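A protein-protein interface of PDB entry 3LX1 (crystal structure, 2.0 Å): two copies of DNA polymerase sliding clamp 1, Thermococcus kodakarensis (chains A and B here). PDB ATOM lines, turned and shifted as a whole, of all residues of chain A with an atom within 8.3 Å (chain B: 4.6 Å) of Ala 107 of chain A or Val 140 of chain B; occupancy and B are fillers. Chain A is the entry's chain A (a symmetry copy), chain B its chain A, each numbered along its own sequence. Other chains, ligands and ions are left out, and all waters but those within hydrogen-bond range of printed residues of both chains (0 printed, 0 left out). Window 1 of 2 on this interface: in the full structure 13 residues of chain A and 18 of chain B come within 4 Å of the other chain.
OE1 of Glu 139 of chain B lies within hydrogen-bond range of OG1 of Thr 106 of chain A (2.9 Å).
NZ of Lys 84 of chain A is in salt-bridge range of OE2 of Glu 143 of chain B.
OE1 of Glu 143 of chain B is in salt-bridge range of NE of Arg 109 of chain A (3.6 Å).
N of Arg 178 of chain B lies within hydrogen-bond range of O of Lys 108 of chain A (3.0 Å).
N of Gly 185 of chain B is in hydrogen-bond range of O of Thr 106 of chain A.
O of Gly 185 of chain B lies within hydrogen-bond range of N of Leu 137 of chain B (2.7 Å).
O of Met 166 of chain B is in hydrogen-bond range of N of Ile 177 of chain B, at 2.8 Å.
The backbone carbonyl oxygen (O) of Arg 82 of chain A sits at hydrogen-bond distance from the guanidinium group (NH1) of Arg 109 of chain A (3.4 Å).
OD2 of Asp 87 of chain A sits at hydrogen-bond distance from N of Lys 84 of chain A.
The side-chain carboxylate (OD2) of Asp 87 of chain A is in salt-bridge range of the guanidinium group (NH2) of Arg 109 of chain A (2.7 Å).
The backbone NH (N) of Phe 103 of chain A lies within hydrogen-bond range of the backbone carbonyl oxygen (O) of Arg 109 of chain A, 2.8 Å away.
O of Glu 143 of chain B touches NH1 of Arg 82 of chain A (3.5 Å).
OG1 of Thr 106 of chain A touches CG2 of Val 140 of chain B (3.3 Å).
Leu 179 of chain B touches Thr 106 of chain A (CD2 to O, 3.8 Å).
CG2 of Val 140 of chain B touches CB of Ala 107 of chain A (3.7 Å).
Leu 179 of chain B touches Ala 107 of chain A.
Ile 177 of chain B touches Lys 108 of chain A.
Arg 109 of chain A touches Ile 177 of chain B (CG to CG1, 3.8 Å).
Ala 107 of chain A touches just these residues of chain B: Val 140 (3.7 Å) and Leu 179 (3.7 Å).
Of the printed residues of chain A, Val 140 of chain B touches Thr 106 and Ala 107.
Printed residues of chain A within 4 Å of Glu 143 of chain B: Arg 82, Lys 84 and Arg 109.
Of the printed residues of chain A, Leu 179 of chain B touches Thr 106 and Ala 107.
Printed residues of chain B within 4 Å of Lys 108 of chain A: Ile 177 and Arg 178.
Of the printed residues of chain A, Gly 185 of chain B touches Thr 106 (2.9 Å).
Of the printed residues of chain B, Arg 109 of chain A touches Glu 143 and Ile 177.
Asp 87 of chain A touches none of the printed residues of chain B.
Gly 138 of chain B touches none of the printed residues of chain A.
The nearest residue of chain B that does not touch Ala 107 of chain A is Arg 178 of chain B (4.1 Å).
The nearest residue of chain A that does not touch Val 140 of chain B is Arg 109 of chain A (5.7 Å).
Of the 14 printed residues of chain B, 7 touch a printed residue of chain A.
Hydrophobic or aromatic side chains of chain B within 4 Å of the printed part of chain A: Val 140, Ile 177 and Leu 179.
Along chain B the printed residues that touch a printed residue of chain A span positions 139 to 185.
Along chain A the printed residues that touch a printed residue of chain B span positions 82 to 109.
Among the printed residues, Asp or Glu carboxylates within 4 Å of a Lys or Arg side-chain nitrogen of the other chain: Lys 84 of chain A with Glu 143 of chain B and Arg 109 of chain A with Glu 143 of chain B.
No position is printed for both chains.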
ATOM      1  N   ARG A  82     -10.929  30.285  -2.903  1.00  0.00           N
ATOM      2  CA  ARG A  82      -9.454  30.302  -2.946  1.00  0.00           C
ATOM      3  C   ARG A  82      -8.952  29.265  -3.951  1.00  0.00           C
ATOM      4  O   ARG A  82      -7.807  29.296  -4.383  1.00  0.00           O
ATOM      5  CB  ARG A  82      -8.908  30.012  -1.528  1.00  0.00           C
ATOM      6  CG  ARG A  82      -9.258  31.110  -0.527  1.00  0.00           C
ATOM      7  CD  ARG A  82      -8.147  32.214  -0.547  1.00  0.00           C
ATOM      8  NE  ARG A  82      -8.149  32.935  -1.799  1.00  0.00           N
ATOM      9  CZ  ARG A  82      -7.194  32.970  -2.716  1.00  0.00           C
ATOM     10  NH1 ARG A  82      -5.992  32.391  -2.592  1.00  0.00           N
ATOM     11  NH2 ARG A  82      -7.484  33.649  -3.794  1.00  0.00           N
ATOM     12  N   LYS A  84      -8.218  27.283  -7.292  1.00  0.00           N
ATOM     13  CA  LYS A  84      -7.976  27.573  -8.706  1.00  0.00           C
ATOM     14  C   LYS A  84      -8.674  26.581  -9.619  1.00  0.00           C
ATOM     15  O   LYS A  84      -9.027  25.473  -9.188  1.00  0.00           O
ATOM     16  CB  LYS A  84      -6.473  27.525  -8.981  1.00  0.00           C
ATOM     17  CG  LYS A  84      -5.752  28.594  -8.259  1.00  0.00           C
ATOM     18  CD  LYS A  84      -4.365  28.837  -8.847  1.00  0.00           C
ATOM     19  CE  LYS A  84      -3.920  30.245  -8.406  1.00  0.00           C
ATOM     20  NZ  LYS A  84      -4.456  30.481  -7.008  1.00  0.00           N
ATOM     21  N   ASP A  87      -6.814  23.448  -9.369  1.00  0.00           N
ATOM     22  CA  ASP A  87      -6.588  22.795  -8.069  1.00  0.00           C
ATOM     23  C   ASP A  87      -7.373  21.516  -7.965  1.00  0.00           C
ATOM     24  O   ASP A  87      -8.455  21.430  -8.471  1.00  0.00           O
ATOM     25  CB  ASP A  87      -6.978  23.699  -6.897  1.00  0.00           C
ATOM     26  CG  ASP A  87      -5.889  24.725  -6.562  1.00  0.00           C
ATOM     27  OD1 ASP A  87      -4.718  24.444  -6.813  1.00  0.00           O
ATOM     28  OD2 ASP A  87      -6.210  25.823  -6.076  1.00  0.00           O
ATOM     29  N   THR A  88      -6.802  20.528  -7.287  1.00  0.00           N
ATOM     30  CA  THR A  88      -7.559  19.422  -6.735  1.00  0.00           C
ATOM     31  C   THR A  88      -8.141  19.738  -5.352  1.00  0.00           C
ATOM     32  O   THR A  88      -7.420  20.196  -4.452  1.00  0.00           O
ATOM     33  CB  THR A  88      -6.654  18.208  -6.634  1.00  0.00           C
ATOM     34  OG1 THR A  88      -6.215  17.897  -7.955  1.00  0.00           O
ATOM     35  CG2 THR A  88      -7.381  16.989  -6.100  1.00  0.00           C
ATOM     36  N   THR A 102      -8.890  21.140   1.523  1.00  0.00           N
ATOM     37  CA  THR A 102      -7.496  21.221   1.068  1.00  0.00           C
ATOM     38  C   THR A 102      -7.471  21.428  -0.462  1.00  0.00           C
ATOM     39  O   THR A 102      -8.204  20.752  -1.232  1.00  0.00           O
ATOM     40  CB  THR A 102      -6.762  19.930   1.429  1.00  0.00           C
ATOM     41  OG1 THR A 102      -6.709  19.748   2.856  1.00  0.00           O
ATOM     42  CG2 THR A 102      -5.398  19.913   0.888  1.00  0.00           C
ATOM     43  N   PHE A 103      -6.638  22.365  -0.901  1.00  0.00           N
ATOM     44  CA  PHE A 103      -6.375  22.563  -2.334  1.00  0.00           C
ATOM     45  C   PHE A 103      -4.970  22.090  -2.627  1.00  0.00           C
ATOM     46  O   PHE A 103      -4.005  22.482  -1.929  1.00  0.00           O
ATOM     47  CB  PHE A 103      -6.527  24.020  -2.750  1.00  0.00           C
ATOM     48  CG  PHE A 103      -7.811  24.651  -2.307  1.00  0.00           C
ATOM     49  CD1 PHE A 103      -9.011  24.367  -2.957  1.00  0.00           C
ATOM     50  CD2 PHE A 103      -7.838  25.543  -1.229  1.00  0.00           C
ATOM     51  CE1 PHE A 103     -10.230  24.940  -2.514  1.00  0.00           C
ATOM     52  CE2 PHE A 103      -9.041  26.114  -0.795  1.00  0.00           C
ATOM     53  CZ  PHE A 103     -10.240  25.824  -1.456  1.00  0.00           C
ATOM     54  N   GLU A 104      -4.851  21.187  -3.603  1.00  0.00           N
ATOM     55  CA  GLU A 104      -3.548  20.678  -4.006  1.00  0.00           C
ATOM     56  C   GLU A 104      -3.245  21.096  -5.434  1.00  0.00           C
ATOM     57  O   GLU A 104      -3.996  20.745  -6.355  1.00  0.00           O
ATOM     58  CB  GLU A 104      -3.473  19.155  -3.887  1.00  0.00           C
ATOM     59  CG  GLU A 104      -3.006  18.672  -2.519  1.00  0.00           C
ATOM     60  CD  GLU A 104      -3.039  17.179  -2.415  1.00  0.00           C
ATOM     61  OE1 GLU A 104      -3.034  16.543  -3.485  1.00  0.00           O
ATOM     62  OE2 GLU A 104      -3.082  16.635  -1.276  1.00  0.00           O
ATOM     63  N   GLY A 105      -2.155  21.859  -5.576  1.00  0.00           N
ATOM     64  CA  GLY A 105      -1.546  22.228  -6.862  1.00  0.00           C
ATOM     65  C   GLY A 105      -0.048  22.099  -6.676  1.00  0.00           C
ATOM     66  O   GLY A 105       0.450  21.016  -6.347  1.00  0.00           O
ATOM     67  N   THR A 106       0.682  23.205  -6.831  1.00  0.00           N
ATOM     68  CA  THR A 106       2.126  23.186  -6.583  1.00  0.00           C
ATOM     69  C   THR A 106       2.454  23.205  -5.079  1.00  0.00           C
ATOM     70  O   THR A 106       3.633  23.056  -4.681  1.00  0.00           O
ATOM     71  CB  THR A 106       2.852  24.347  -7.324  1.00  0.00           C
ATOM     72  OG1 THR A 106       2.323  25.600  -6.859  1.00  0.00           O
ATOM     73  CG2 THR A 106       2.613  24.249  -8.855  1.00  0.00           C
ATOM     74  N   ALA A 107       1.420  23.407  -4.250  1.00  0.00           N
ATOM     75  CA  ALA A 107       1.527  23.309  -2.789  1.00  0.00           C
ATOM     76  C   ALA A 107       0.227  22.704  -2.253  1.00  0.00           C
ATOM     77  O   ALA A 107      -0.770  22.614  -2.992  1.00  0.00           O
ATOM     78  CB  ALA A 107       1.764  24.696  -2.158  1.00  0.00           C
ATOM     79  N   LYS A 108       0.247  22.287  -0.990  1.00  0.00           N
ATOM     80  CA  LYS A 108      -0.940  21.728  -0.313  1.00  0.00           C
ATOM     81  C   LYS A 108      -1.412  22.752   0.714  1.00  0.00           C
ATOM     82  O   LYS A 108      -0.657  23.117   1.648  1.00  0.00           O
ATOM     83  CB  LYS A 108      -0.602  20.375   0.326  1.00  0.00           C
ATOM     84  CG  LYS A 108      -1.686  19.833   1.254  1.00  0.00           C
ATOM     85  CD  LYS A 108      -1.242  18.573   2.062  1.00  0.00           C
ATOM     86  CE  LYS A 108      -1.971  18.522   3.411  1.00  0.00           C
ATOM     87  NZ  LYS A 108      -2.134  17.099   3.982  1.00  0.00           N
ATOM     88  N   ARG A 109      -2.622  23.275   0.509  1.00  0.00           N
ATOM     89  CA  ARG A 109      -3.164  24.370   1.326  1.00  0.00           C
ATOM     90  C   ARG A 109      -4.452  23.886   1.998  1.00  0.00           C
ATOM     91  O   ARG A 109      -5.478  23.593   1.301  1.00  0.00           O
ATOM     92  CB  ARG A 109      -3.506  25.598   0.501  1.00  0.00           C
ATOM     93  CG  ARG A 109      -2.415  26.157  -0.383  1.00  0.00           C
ATOM     94  CD  ARG A 109      -2.966  27.378  -1.065  1.00  0.00           C
ATOM     95  NE  ARG A 109      -3.634  26.990  -2.271  1.00  0.00           N
ATOM     96  CZ  ARG A 109      -4.641  27.617  -2.860  1.00  0.00           C
ATOM     97  NH1 ARG A 109      -5.192  28.703  -2.373  1.00  0.00           N
ATOM     98  NH2 ARG A 109      -5.105  27.104  -3.980  1.00  0.00           N
ATOM     99  N   THR A 110      -4.415  23.846   3.324  1.00  0.00           N
ATOM    100  CA  THR A 110      -5.475  23.208   4.074  1.00  0.00           C
ATOM    101  C   THR A 110      -6.157  24.187   4.974  1.00  0.00           C
ATOM    102  O   THR A 110      -5.500  24.803   5.799  1.00  0.00           O
ATOM    103  CB  THR A 110      -4.958  22.053   4.922  1.00  0.00           C
ATOM    104  OG1 THR A 110      -4.543  21.015   4.034  1.00  0.00           O
ATOM    105  CG2 THR A 110      -6.074  21.524   5.821  1.00  0.00           C
ATOM    106  N   LEU B 136      10.863  29.785  -3.111  1.00  0.00           N
ATOM    107  CA  LEU B 136       9.643  29.120  -3.552  1.00  0.00           C
ATOM    108  C   LEU B 136       9.086  29.757  -4.804  1.00  0.00           C
ATOM    109  O   LEU B 136       9.477  30.883  -5.160  1.00  0.00           O
ATOM    110  CB  LEU B 136       8.622  29.010  -2.399  1.00  0.00           C
ATOM    111  CG  LEU B 136       8.145  30.240  -1.643  1.00  0.00           C
ATOM    112  CD1 LEU B 136       7.399  30.965  -2.600  1.00  0.00           C
ATOM    113  CD2 LEU B 136       7.187  29.936  -0.492  1.00  0.00           C
ATOM    114  N   LEU B 137       8.177  29.053  -5.483  1.00  0.00           N
ATOM    115  CA  LEU B 137       7.524  29.577  -6.664  1.00  0.00           C
ATOM    116  C   LEU B 137       6.599  30.673  -6.267  1.00  0.00           C
ATOM    117  O   LEU B 137       5.879  30.560  -5.251  1.00  0.00           O
ATOM    118  CB  LEU B 137       6.707  28.476  -7.353  1.00  0.00           C
ATOM    119  CG  LEU B 137       7.183  27.708  -8.579  1.00  0.00           C
ATOM    120  CD1 LEU B 137       5.946  26.910  -9.050  1.00  0.00           C
ATOM    121  CD2 LEU B 137       7.741  28.613  -9.714  1.00  0.00           C
ATOM    122  N   GLY B 138       6.580  31.739  -7.073  1.00  0.00           N
ATOM    123  CA  GLY B 138       5.761  32.915  -6.828  1.00  0.00           C
ATOM    124  C   GLY B 138       4.305  32.617  -6.569  1.00  0.00           C
ATOM    125  O   GLY B 138       3.666  33.270  -5.766  1.00  0.00           O
ATOM    126  N   GLU B 139       3.781  31.611  -7.248  1.00  0.00           N
ATOM    127  CA  GLU B 139       2.351  31.320  -7.190  1.00  0.00           C
ATOM    128  C   GLU B 139       1.956  30.877  -5.761  1.00  0.00           C
ATOM    129  O   GLU B 139       0.931  31.310  -5.241  1.00  0.00           O
ATOM    130  CB  GLU B 139       2.034  30.276  -8.267  1.00  0.00           C
ATOM    131  CG  GLU B 139       0.909  29.306  -7.973  1.00  0.00           C
ATOM    132  CD  GLU B 139       0.722  28.319  -9.108  1.00  0.00           C
ATOM    133  OE1 GLU B 139       1.424  27.267  -9.112  1.00  0.00           O
ATOM    134  OE2 GLU B 139      -0.129  28.622 -10.000  1.00  0.00           O
ATOM    135  N   VAL B 140       2.815  30.088  -5.126  1.00  0.00           N
ATOM    136  CA  VAL B 140       2.573  29.546  -3.767  1.00  0.00           C
ATOM    137  C   VAL B 140       2.510  30.628  -2.702  1.00  0.00           C
ATOM    138  O   VAL B 140       1.640  30.637  -1.786  1.00  0.00           O
ATOM    139  CB  VAL B 140       3.659  28.555  -3.427  1.00  0.00           C
ATOM    140  CG1 VAL B 140       3.647  28.229  -1.934  1.00  0.00           C
ATOM    141  CG2 VAL B 140       3.399  27.305  -4.209  1.00  0.00           C
ATOM    142  N   LEU B 141       3.426  31.581  -2.839  1.00  0.00           N
ATOM    143  CA  LEU B 141       3.514  32.645  -1.892  1.00  0.00           C
ATOM    144  C   LEU B 141       2.339  33.555  -2.083  1.00  0.00           C
ATOM    145  O   LEU B 141       1.725  33.956  -1.125  1.00  0.00           O
ATOM    146  CB  LEU B 141       4.878  33.391  -2.068  1.00  0.00           C
ATOM    147  CG  LEU B 141       5.282  34.425  -1.038  1.00  0.00           C
ATOM    148  CD1 LEU B 141       5.334  33.909   0.402  1.00  0.00           C
ATOM    149  CD2 LEU B 141       6.644  35.110  -1.458  1.00  0.00           C
ATOM    150  N   LYS B 142       1.991  33.875  -3.333  1.00  0.00           N
ATOM    151  CA  LYS B 142       0.847  34.778  -3.575  1.00  0.00           C
ATOM    152  C   LYS B 142      -0.453  34.146  -3.089  1.00  0.00           C
ATOM    153  O   LYS B 142      -1.241  34.808  -2.463  1.00  0.00           O
ATOM    154  CB  LYS B 142       0.706  35.154  -5.069  1.00  0.00           C
ATOM    155  CG  LYS B 142       1.871  35.888  -5.699  1.00  0.00           C
ATOM    156  CD  LYS B 142       1.852  35.803  -7.272  1.00  0.00           C
ATOM    157  CE  LYS B 142       0.697  36.601  -7.955  1.00  0.00           C
ATOM    158  NZ  LYS B 142       0.870  38.123  -7.832  1.00  0.00           N
ATOM    159  N   GLU B 143      -0.673  32.872  -3.404  1.00  0.00           N
ATOM    160  CA  GLU B 143      -1.843  32.062  -2.911  1.00  0.00           C
ATOM    161  C   GLU B 143      -1.908  32.002  -1.412  1.00  0.00           C
ATOM    162  O   GLU B 143      -2.956  32.272  -0.795  1.00  0.00           O
ATOM    163  CB  GLU B 143      -1.672  30.603  -3.325  1.00  0.00           C
ATOM    164  CG  GLU B 143      -2.113  30.273  -4.691  1.00  0.00           C
ATOM    165  CD  GLU B 143      -1.760  28.818  -5.086  1.00  0.00           C
ATOM    166  OE1 GLU B 143      -0.970  28.086  -4.415  1.00  0.00           O
ATOM    167  OE2 GLU B 143      -2.279  28.425  -6.123  1.00  0.00           O
ATOM    168  N   GLY B 144      -0.785  31.599  -0.818  1.00  0.00           N
ATOM    169  CA  GLY B 144      -0.716  31.450   0.646  1.00  0.00           C
ATOM    170  C   GLY B 144      -1.056  32.708   1.441  1.00  0.00           C
ATOM    171  O   GLY B 144      -1.790  32.651   2.460  1.00  0.00           O
ATOM    172  N   MET B 166       3.582  27.961   6.248  1.00  0.00           N
ATOM    173  CA  MET B 166       2.925  29.213   6.645  1.00  0.00           C
ATOM    174  C   MET B 166       1.562  28.859   7.291  1.00  0.00           C
ATOM    175  O   MET B 166       0.788  28.079   6.751  1.00  0.00           O
ATOM    176  CB  MET B 166       2.701  30.096   5.425  1.00  0.00           C
ATOM    177  CG  MET B 166       4.005  30.320   4.622  1.00  0.00           C
ATOM    178  SD  MET B 166       3.675  31.401   3.226  1.00  0.00           S
ATOM    179  CE  MET B 166       3.109  30.225   2.065  1.00  0.00           C
ATOM    180  N   ILE B 177      -0.400  26.337   4.930  1.00  0.00           N
ATOM    181  CA  ILE B 177       0.199  26.103   3.600  1.00  0.00           C
ATOM    182  C   ILE B 177       1.513  25.402   3.815  1.00  0.00           C
ATOM    183  O   ILE B 177       2.430  25.918   4.471  1.00  0.00           O
ATOM    184  CB  ILE B 177       0.358  27.348   2.735  1.00  0.00           C
ATOM    185  CG1 ILE B 177      -0.988  28.083   2.556  1.00  0.00           C
ATOM    186  CG2 ILE B 177       0.926  26.970   1.350  1.00  0.00           C
ATOM    187  CD1 ILE B 177      -1.294  29.246   3.577  1.00  0.00           C
ATOM    188  N   ARG B 178       1.601  24.192   3.310  1.00  0.00           N
ATOM    189  CA  ARG B 178       2.789  23.419   3.551  1.00  0.00           C
ATOM    190  C   ARG B 178       3.531  22.964   2.280  1.00  0.00           C
ATOM    191  O   ARG B 178       2.933  22.733   1.191  1.00  0.00           O
ATOM    192  CB  ARG B 178       2.537  22.253   4.505  1.00  0.00           C
ATOM    193  CG  ARG B 178       3.696  21.248   4.458  1.00  0.00           C
ATOM    194  CD  ARG B 178       3.835  20.467   5.721  1.00  0.00           C
ATOM    195  NE  ARG B 178       3.522  21.305   6.873  1.00  0.00           N
ATOM    196  CZ  ARG B 178       3.301  20.841   8.105  1.00  0.00           C
ATOM    197  NH1 ARG B 178       3.374  19.527   8.346  1.00  0.00           N
ATOM    198  NH2 ARG B 178       3.014  21.689   9.095  1.00  0.00           N
ATOM    199  N   LEU B 179       4.840  22.872   2.454  1.00  0.00           N
ATOM    200  CA  LEU B 179       5.768  22.660   1.385  1.00  0.00           C
ATOM    201  C   LEU B 179       6.915  21.833   1.899  1.00  0.00           C
ATOM    202  O   LEU B 179       7.530  22.171   2.900  1.00  0.00           O
ATOM    203  CB  LEU B 179       6.301  24.002   0.902  1.00  0.00           C
ATOM    204  CG  LEU B 179       5.386  24.731  -0.061  1.00  0.00           C
ATOM    205  CD1 LEU B 179       5.901  26.117  -0.188  1.00  0.00           C
ATOM    206  CD2 LEU B 179       5.337  24.071  -1.414  1.00  0.00           C
ATOM    207  N   GLY B 185       6.268  23.616  -5.735  1.00  0.00           N
ATOM    208  CA  GLY B 185       6.328  24.989  -5.197  1.00  0.00           C
ATOM    209  C   GLY B 185       7.658  25.368  -4.525  1.00  0.00           C
ATOM    210  O   GLY B 185       7.994  26.540  -4.471  1.00  0.00           O
